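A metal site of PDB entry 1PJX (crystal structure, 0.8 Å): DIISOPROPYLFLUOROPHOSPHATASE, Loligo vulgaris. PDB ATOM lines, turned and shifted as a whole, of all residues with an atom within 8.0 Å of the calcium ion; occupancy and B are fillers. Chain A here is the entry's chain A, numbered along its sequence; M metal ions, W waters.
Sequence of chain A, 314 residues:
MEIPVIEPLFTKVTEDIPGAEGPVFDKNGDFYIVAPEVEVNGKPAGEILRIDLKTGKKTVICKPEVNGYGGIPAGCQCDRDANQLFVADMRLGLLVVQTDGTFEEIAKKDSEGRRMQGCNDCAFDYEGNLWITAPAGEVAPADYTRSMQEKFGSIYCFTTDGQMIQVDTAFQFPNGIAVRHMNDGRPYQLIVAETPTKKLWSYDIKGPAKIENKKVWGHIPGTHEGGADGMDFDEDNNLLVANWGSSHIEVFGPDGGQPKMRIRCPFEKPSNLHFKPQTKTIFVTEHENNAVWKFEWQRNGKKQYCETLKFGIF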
ATOM      1  N   GLY A  19     -23.787 -19.677  15.612  1.00  0.00           N
ATOM      2  CA  GLY A  19     -22.491 -20.316  15.665  1.00  0.00           C
ATOM      3  C   GLY A  19     -22.518 -21.814  15.650  1.00  0.00           C
ATOM      4  O   GLY A  19     -21.563 -22.449  16.079  1.00  0.00           O
ATOM      5  N   ALA A  20     -23.588 -22.410  15.077  1.00  0.00           N
ATOM      6  CA  ALA A  20     -23.844 -23.821  15.029  1.00  0.00           C
ATOM      7  C   ALA A  20     -22.533 -24.604  14.901  1.00  0.00           C
ATOM      8  O   ALA A  20     -21.780 -24.444  13.932  1.00  0.00           O
ATOM      9  CB  ALA A  20     -24.744 -24.146  13.845  1.00  0.00           C
ATOM     10  N   GLU A  21     -22.345 -25.537  15.828  1.00  0.00           N
ATOM     11  CA  GLU A  21     -21.055 -26.183  16.053  1.00  0.00           C
ATOM     12  C   GLU A  21     -21.253 -27.553  16.630  1.00  0.00           C
ATOM     13  O   GLU A  21     -22.366 -27.999  16.987  1.00  0.00           O
ATOM     14  CB  GLU A  21     -20.164 -25.317  16.975  1.00  0.00           C
ATOM     15  CG  GLU A  21     -19.057 -24.548  16.266  1.00  0.00           C
ATOM     16  CD  GLU A  21     -17.854 -25.380  15.960  1.00  0.00           C
ATOM     17  OE1 GLU A  21     -17.990 -26.643  15.818  1.00  0.00           O
ATOM     18  OE2 GLU A  21     -16.763 -24.773  15.887  1.00  0.00           O
ATOM     19  N   GLY A  22     -20.133 -28.275  16.755  1.00  0.00           N
ATOM     20  CA  GLY A  22     -20.036 -29.489  17.487  1.00  0.00           C
ATOM     21  C   GLY A  22     -21.121 -30.542  17.244  1.00  0.00           C
ATOM     22  O   GLY A  22     -21.634 -31.124  18.196  1.00  0.00           O
ATOM     23  N   PRO A  36     -22.642 -21.966  20.348  1.00  0.00           N
ATOM     24  CA  PRO A  36     -21.724 -21.254  21.206  1.00  0.00           C
ATOM     25  C   PRO A  36     -22.036 -19.796  21.299  1.00  0.00           C
ATOM     26  O   PRO A  36     -21.676 -19.176  22.334  1.00  0.00           O
ATOM     27  CB  PRO A  36     -20.349 -21.444  20.531  1.00  0.00           C
ATOM     28  CG  PRO A  36     -20.663 -21.988  19.154  1.00  0.00           C
ATOM     29  CD  PRO A  36     -21.947 -22.738  19.311  1.00  0.00           C
ATOM     30  N   ALA A  74     -18.661 -25.247  22.149  1.00  0.00           N
ATOM     31  CA  ALA A  74     -18.233 -25.175  20.756  1.00  0.00           C
ATOM     32  C   ALA A  74     -17.911 -26.507  20.088  1.00  0.00           C
ATOM     33  O   ALA A  74     -17.871 -26.531  18.857  1.00  0.00           O
ATOM     34  CB  ALA A  74     -17.094 -24.204  20.557  1.00  0.00           C
ATOM     35  N   GLY A  75     -17.655 -27.572  20.830  1.00  0.00           N
ATOM     36  CA  GLY A  75     -17.266 -28.818  20.210  1.00  0.00           C
ATOM     37  C   GLY A  75     -17.599 -29.978  21.110  1.00  0.00           C
ATOM     38  O   GLY A  75     -17.619 -29.823  22.341  1.00  0.00           O
ATOM     39  N   MET A  90     -15.490 -22.422  25.211  1.00  0.00           N
ATOM     40  CA  MET A  90     -14.522 -21.362  25.097  1.00  0.00           C
ATOM     41  C   MET A  90     -14.402 -20.485  26.355  1.00  0.00           C
ATOM     42  O   MET A  90     -13.416 -19.786  26.502  1.00  0.00           O
ATOM     43  CB  MET A  90     -14.831 -20.456  23.896  1.00  0.00           C
ATOM     44  CG  MET A  90     -14.708 -21.166  22.571  1.00  0.00           C
ATOM     45  SD  MET A  90     -12.975 -21.281  21.995  1.00  0.00           S
ATOM     46  CE  MET A  90     -12.730 -19.587  21.429  1.00  0.00           C
ATOM     47  N   CYS A 119     -11.743 -23.914  25.498  1.00  0.00           N
ATOM     48  CA  CYS A 119     -11.565 -24.948  24.491  1.00  0.00           C
ATOM     49  C   CYS A 119     -12.585 -24.822  23.365  1.00  0.00           C
ATOM     50  O   CYS A 119     -13.654 -24.236  23.530  1.00  0.00           O
ATOM     51  CB  CYS A 119     -11.649 -26.296  25.145  1.00  0.00           C
ATOM     52  SG  CYS A 119     -10.330 -26.593  26.357  1.00  0.00           S
ATOM     53  N   ASN A 120     -12.216 -25.387  22.208  1.00  0.00           N
ATOM     54  CA  ASN A 120     -13.073 -25.307  21.029  1.00  0.00           C
ATOM     55  C   ASN A 120     -13.513 -26.637  20.461  1.00  0.00           C
ATOM     56  O   ASN A 120     -14.683 -26.779  20.102  1.00  0.00           O
ATOM     57  CB  ASN A 120     -12.455 -24.410  19.930  1.00  0.00           C
ATOM     58  CG  ASN A 120     -13.480 -24.018  18.869  1.00  0.00           C
ATOM     59  OD1 ASN A 120     -13.759 -24.767  17.930  1.00  0.00           O
ATOM     60  ND2 ASN A 120     -14.106 -22.849  19.041  1.00  0.00           N
ATOM     61  N   ASP A 121     -12.601 -27.609  20.331  1.00  0.00           N
ATOM     62  CA  ASP A 121     -13.003 -28.912  19.819  1.00  0.00           C
ATOM     63  C   ASP A 121     -12.205 -29.986  20.512  1.00  0.00           C
ATOM     64  O   ASP A 121     -11.219 -29.725  21.227  1.00  0.00           O
ATOM     65  CB  ASP A 121     -12.912 -28.968  18.277  1.00  0.00           C
ATOM     66  CG  ASP A 121     -13.930 -29.889  17.622  1.00  0.00           C
ATOM     67  OD1 ASP A 121     -14.633 -30.649  18.337  1.00  0.00           O
ATOM     68  OD2 ASP A 121     -14.018 -29.841  16.356  1.00  0.00           O
ATOM     69  N   CYS A 122     -12.631 -31.236  20.319  1.00  0.00           N
ATOM     70  CA  CYS A 122     -11.974 -32.350  20.972  1.00  0.00           C
ATOM     71  C   CYS A 122     -12.171 -33.628  20.148  1.00  0.00           C
ATOM     72  O   CYS A 122     -13.109 -33.733  19.350  1.00  0.00           O
ATOM     73  CB  CYS A 122     -12.372 -32.484  22.447  1.00  0.00           C
ATOM     74  SG  CYS A 122     -14.137 -32.753  22.743  1.00  0.00           S
ATOM     75  N   THR A 133      -8.449 -28.871  21.648  1.00  0.00           N
ATOM     76  CA  THR A 133      -7.899 -27.590  21.267  1.00  0.00           C
ATOM     77  C   THR A 133      -8.419 -26.510  22.166  1.00  0.00           C
ATOM     78  O   THR A 133      -9.590 -26.474  22.547  1.00  0.00           O
ATOM     79  CB  THR A 133      -8.200 -27.255  19.818  1.00  0.00           C
ATOM     80  OG1 THR A 133      -9.620 -27.212  19.661  1.00  0.00           O
ATOM     81  CG2 THR A 133      -7.554 -28.252  18.884  1.00  0.00           C
ATOM     82  N   PRO A 135      -8.172 -22.570  21.943  1.00  0.00           N
ATOM     83  CA  PRO A 135      -7.802 -21.317  21.306  1.00  0.00           C
ATOM     84  C   PRO A 135      -8.154 -20.075  22.119  1.00  0.00           C
ATOM     85  O   PRO A 135      -7.712 -18.980  21.741  1.00  0.00           O
ATOM     86  CB  PRO A 135      -8.562 -21.345  19.980  1.00  0.00           C
ATOM     87  CG  PRO A 135      -9.838 -22.111  20.314  1.00  0.00           C
ATOM     88  CD  PRO A 135      -9.380 -23.168  21.291  1.00  0.00           C
ATOM     89  N   PHE A 173      -5.040 -19.929  17.132  1.00  0.00           N
ATOM     90  CA  PHE A 173      -6.396 -20.465  16.980  1.00  0.00           C
ATOM     91  C   PHE A 173      -6.420 -21.916  16.535  1.00  0.00           C
ATOM     92  O   PHE A 173      -6.925 -22.303  15.479  1.00  0.00           O
ATOM     93  CB  PHE A 173      -7.335 -19.582  16.106  1.00  0.00           C
ATOM     94  CG  PHE A 173      -8.740 -19.655  16.644  1.00  0.00           C
ATOM     95  CD1 PHE A 173      -9.605 -20.676  16.304  1.00  0.00           C
ATOM     96  CD2 PHE A 173      -9.200 -18.712  17.550  1.00  0.00           C
ATOM     97  CE1 PHE A 173     -10.876 -20.734  16.821  1.00  0.00           C
ATOM     98  CE2 PHE A 173     -10.466 -18.782  18.054  1.00  0.00           C
ATOM     99  CZ  PHE A 173     -11.304 -19.800  17.724  1.00  0.00           C
ATOM    100  N   PRO A 174      -5.893 -22.808  17.407  1.00  0.00           N
ATOM    101  CA  PRO A 174      -6.100 -24.241  17.182  1.00  0.00           C
ATOM    102  C   PRO A 174      -7.627 -24.537  17.255  1.00  0.00           C
ATOM    103  O   PRO A 174      -8.309 -23.990  18.107  1.00  0.00           O
ATOM    104  CB  PRO A 174      -5.328 -24.889  18.335  1.00  0.00           C
ATOM    105  CG  PRO A 174      -5.437 -23.852  19.464  1.00  0.00           C
ATOM    106  CD  PRO A 174      -5.345 -22.549  18.733  1.00  0.00           C
ATOM    107  N   ASN A 175      -8.088 -25.412  16.350  1.00  0.00           N
ATOM    108  CA  ASN A 175      -9.519 -25.477  16.097  1.00  0.00           C
ATOM    109  C   ASN A 175      -9.960 -26.920  16.008  1.00  0.00           C
ATOM    110  O   ASN A 175     -10.043 -27.638  17.022  1.00  0.00           O
ATOM    111  CB  ASN A 175      -9.891 -24.570  14.948  1.00  0.00           C
ATOM    112  CG  ASN A 175     -11.362 -24.226  14.942  1.00  0.00           C
ATOM    113  OD1 ASN A 175     -12.137 -24.967  15.555  1.00  0.00           O
ATOM    114  ND2 ASN A 175     -11.736 -23.149  14.300  1.00  0.00           N
ATOM    115  N   GLY A 176     -10.182 -27.476  14.800  1.00  0.00           N
ATOM    116  CA  GLY A 176     -10.468 -28.874  14.687  1.00  0.00           C
ATOM    117  C   GLY A 176      -9.282 -29.742  15.084  1.00  0.00           C
ATOM    118  O   GLY A 176      -8.111 -29.315  15.102  1.00  0.00           O
ATOM    119  N   ILE A 177      -9.612 -30.989  15.390  1.00  0.00           N
ATOM    120  CA  ILE A 177      -8.632 -31.961  15.863  1.00  0.00           C
ATOM    121  C   ILE A 177      -9.168 -33.337  15.534  1.00  0.00           C
ATOM    122  O   ILE A 177     -10.389 -33.561  15.575  1.00  0.00           O
ATOM    123  CB  ILE A 177      -8.346 -31.721  17.361  1.00  0.00           C
ATOM    124  CG1 ILE A 177      -7.193 -32.580  17.896  1.00  0.00           C
ATOM    125  CG2 ILE A 177      -9.594 -31.811  18.226  1.00  0.00           C
ATOM    126  CD1 ILE A 177      -6.606 -32.010  19.194  1.00  0.00           C
ATOM    127  N   ALA A 193      -5.989 -28.429  13.370  1.00  0.00           N
ATOM    128  CA  ALA A 193      -6.162 -27.277  12.525  1.00  0.00           C
ATOM    129  C   ALA A 193      -5.703 -26.007  13.224  1.00  0.00           C
ATOM    130  O   ALA A 193      -6.011 -25.798  14.410  1.00  0.00           O
ATOM    131  CB  ALA A 193      -7.643 -27.112  12.173  1.00  0.00           C
ATOM    132  N   THR A 195      -6.492 -22.257  12.460  1.00  0.00           N
ATOM    133  CA  THR A 195      -7.433 -21.684  11.484  1.00  0.00           C
ATOM    134  C   THR A 195      -6.813 -20.621  10.579  1.00  0.00           C
ATOM    135  O   THR A 195      -6.736 -20.844   9.350  1.00  0.00           O
ATOM    136  CB  THR A 195      -8.718 -21.218  12.167  1.00  0.00           C
ATOM    137  OG1 THR A 195      -9.331 -22.351  12.809  1.00  0.00           O
ATOM    138  CG2 THR A 195      -9.663 -20.563  11.207  1.00  0.00           C
ATOM    139  N   ALA A 228      -9.262 -23.749   8.225  1.00  0.00           N
ATOM    140  CA  ALA A 228      -9.795 -25.011   8.708  1.00  0.00           C
ATOM    141  C   ALA A 228     -10.457 -24.844  10.079  1.00  0.00           C
ATOM    142  O   ALA A 228      -9.861 -24.263  11.004  1.00  0.00           O
ATOM    143  CB  ALA A 228      -8.666 -26.031   8.869  1.00  0.00           C
ATOM    144  N   ASP A 229     -11.655 -25.393  10.186  1.00  0.00           N
ATOM    145  CA  ASP A 229     -12.437 -25.404  11.421  1.00  0.00           C
ATOM    146  C   ASP A 229     -12.518 -26.858  11.872  1.00  0.00           C
ATOM    147  O   ASP A 229     -11.523 -27.387  12.361  1.00  0.00           O
ATOM    148  CB  ASP A 229     -13.733 -24.635  11.232  1.00  0.00           C
ATOM    149  CG  ASP A 229     -14.547 -24.453  12.496  1.00  0.00           C
ATOM    150  OD1 ASP A 229     -14.264 -25.219  13.461  1.00  0.00           O
ATOM    151  OD2 ASP A 229     -15.452 -23.589  12.521  1.00  0.00           O
ATOM    152  N   GLY A 230     -13.628 -27.549  11.651  1.00  0.00           N
ATOM    153  CA  GLY A 230     -13.786 -28.895  12.129  1.00  0.00           C
ATOM    154  C   GLY A 230     -13.356 -29.965  11.160  1.00  0.00           C
ATOM    155  O   GLY A 230     -13.300 -29.746   9.942  1.00  0.00           O
ATOM    156  N   MET A 231     -13.114 -31.159  11.664  1.00  0.00           N
ATOM    157  CA  MET A 231     -12.612 -32.244  10.841  1.00  0.00           C
ATOM    158  C   MET A 231     -13.052 -33.600  11.356  1.00  0.00           C
ATOM    159  O   MET A 231     -13.338 -33.781  12.558  1.00  0.00           O
ATOM    160  CB  MET A 231     -11.077 -32.210  10.757  1.00  0.00           C
ATOM    161  CG  MET A 231     -10.431 -32.420  12.072  1.00  0.00           C
ATOM    162  SD  MET A 231      -8.605 -32.388  12.038  1.00  0.00           S
ATOM    163  CE  MET A 231      -8.391 -30.766  11.338  1.00  0.00           C
ATOM    164  N   TRP A 244     -13.714 -22.876   6.601  1.00  0.00           N
ATOM    165  CA  TRP A 244     -14.624 -21.800   6.898  1.00  0.00           C
ATOM    166  C   TRP A 244     -14.201 -20.568   6.092  1.00  0.00           C
ATOM    167  O   TRP A 244     -13.055 -20.116   6.198  1.00  0.00           O
ATOM    168  CB  TRP A 244     -14.586 -21.510   8.410  1.00  0.00           C
ATOM    169  CG  TRP A 244     -15.613 -20.590   8.968  1.00  0.00           C
ATOM    170  CD1 TRP A 244     -16.618 -20.975   9.779  1.00  0.00           C
ATOM    171  CD2 TRP A 244     -15.622 -19.164   8.974  1.00  0.00           C
ATOM    172  NE1 TRP A 244     -17.292 -19.922  10.287  1.00  0.00           N
ATOM    173  CE2 TRP A 244     -16.679 -18.745   9.830  1.00  0.00           C
ATOM    174  CE3 TRP A 244     -14.848 -18.148   8.411  1.00  0.00           C
ATOM    175  CZ2 TRP A 244     -16.937 -17.437  10.146  1.00  0.00           C
ATOM    176  CZ3 TRP A 244     -15.107 -16.820   8.726  1.00  0.00           C
ATOM    177  CH2 TRP A 244     -16.129 -16.479   9.584  1.00  0.00           C
ATOM    178  N   SER A 271     -18.476 -24.992   9.191  1.00  0.00           N
ATOM    179  CA  SER A 271     -17.788 -24.942  10.459  1.00  0.00           C
ATOM    180  C   SER A 271     -17.403 -26.311  10.957  1.00  0.00           C
ATOM    181  O   SER A 271     -16.228 -26.600  11.201  1.00  0.00           O
ATOM    182  CB  SER A 271     -18.637 -24.218  11.497  1.00  0.00           C
ATOM    183  OG  SER A 271     -18.123 -24.386  12.770  1.00  0.00           O
ATOM    184  N   ASN A 272     -18.328 -27.229  11.070  1.00  0.00           N
ATOM    185  CA  ASN A 272     -17.989 -28.503  11.659  1.00  0.00           C
ATOM    186  C   ASN A 272     -18.852 -29.594  11.046  1.00  0.00           C
ATOM    187  O   ASN A 272     -19.823 -29.314  10.326  1.00  0.00           O
ATOM    188  CB  ASN A 272     -18.040 -28.446  13.192  1.00  0.00           C
ATOM    189  CG  ASN A 272     -17.025 -29.362  13.854  1.00  0.00           C
ATOM    190  OD1 ASN A 272     -16.546 -30.319  13.264  1.00  0.00           O
ATOM    191  ND2 ASN A 272     -16.629 -28.997  15.076  1.00  0.00           N
ATOM    192  N   THR A 285     -22.442 -28.175  10.001  1.00  0.00           N
ATOM    193  CA  THR A 285     -22.893 -26.929  10.538  1.00  0.00           C
ATOM    194  C   THR A 285     -22.238 -25.785   9.753  1.00  0.00           C
ATOM    195  O   THR A 285     -21.135 -25.955   9.228  1.00  0.00           O
ATOM    196  CB  THR A 285     -22.583 -26.808  12.037  1.00  0.00           C
ATOM    197  OG1 THR A 285     -21.190 -26.698  12.236  1.00  0.00           O
ATOM    198  CG2 THR A 285     -23.146 -27.926  12.832  1.00  0.00           C
ATOM    199  N   HIS A 287     -22.024 -21.172   9.289  1.00  0.00           N
ATOM    200  CA  HIS A 287     -22.187 -19.896   9.919  1.00  0.00           C
ATOM    201  C   HIS A 287     -22.609 -18.762   8.994  1.00  0.00           C
ATOM    202  O   HIS A 287     -22.672 -17.620   9.389  1.00  0.00           O
ATOM    203  CB  HIS A 287     -20.944 -19.497  10.685  1.00  0.00           C
ATOM    204  CG  HIS A 287     -20.564 -20.479  11.781  1.00  0.00           C
ATOM    205  ND1 HIS A 287     -19.335 -20.396  12.375  1.00  0.00           N
ATOM    206  CD2 HIS A 287     -21.252 -21.505  12.293  1.00  0.00           C
ATOM    207  CE1 HIS A 287     -19.322 -21.403  13.237  1.00  0.00           C
ATOM    208  NE2 HIS A 287     -20.454 -22.078  13.225  1.00  0.00           N
HETATM  209 CA    CA M   1     -14.490 -25.368  15.802  1.00  0.00          CA
HETATM  210  O   HOH W   1     -15.478 -26.987  17.385  1.00  0.00           O
HETATM  211  O   HOH W   2     -13.570 -27.440  15.210  1.00  0.00           O
HETATM  212  O   HOH W   3     -14.582 -22.945  15.124  1.00  0.00           O
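The backbone carbonyl oxygen of Thr 133 is in hydrogen-bond range of the backbone NH of Asn 120 (2.9 Å).
The side-chain amide nitrogen of Asn 175 is in hydrogen-bond range of the side-chain hydroxyl of Thr 195 (2.9 Å).
The backbone NH of Gly 75 is in hydrogen-bond range of the backbone carbonyl oxygen of Asn 120 (3.2 Å).
O of Asn 175 lies within hydrogen-bond range of OG1 of Thr 133, 2.7 Å away.
OE1 of Glu 21 sits at hydrogen-bond distance from ND2 of Asn 272 (2.8 Å).
The side-chain sulfur (SD) of Met 90 is in hydrogen-bond range of the side-chain amide nitrogen (ND2) of Asn 120, 3.5 Å away.
The side-chain carboxylate (OE2) of Glu 21 sits close to the side-chain hydroxyl (OG) of Ser 271 (3.4 Å).
The backbone carbonyl oxygen (O) of Asp 229 lies within hydrogen-bond range of the backbone NH (N) of Gly 176 (2.8 Å).
Four residues have an atom within 4 Å of the calcium ion: Glu 21, Asn 120, Asn 175 and Asp 229.
The nearest printed residue that does not touch the calcium ion is Asn 272 (4.3 Å).
The side-chain amide oxygen (OD1) of Asn 120 binds the calcium ion, 2.3 Å away.
The calcium ion is bound by water W2 (2.3 Å).
OE2 of Glu 21 binds the calcium ion, at 2.4 Å.
OD1 of Asp 229 is bound to the calcium ion.
The calcium ion is bound by the side-chain amide oxygen (OD1) of Asn 175, 2.4 Å away.
The calcium ion is bound by water W1 (2.5 Å).
Water W3 is bound to the calcium ion, 2.5 Å away.
Water W2 lies within hydrogen-bond range of the side-chain carboxylate of Asp 121, the backbone NH of Gly 176 and the side-chain amide nitrogen of Asn 272.
Water W3 bridges the side-chain carboxylate (OD2) of Asp 229 (2.8 Å) and the side-chain amide nitrogen (ND2) of Asn 175 (3.0 Å).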
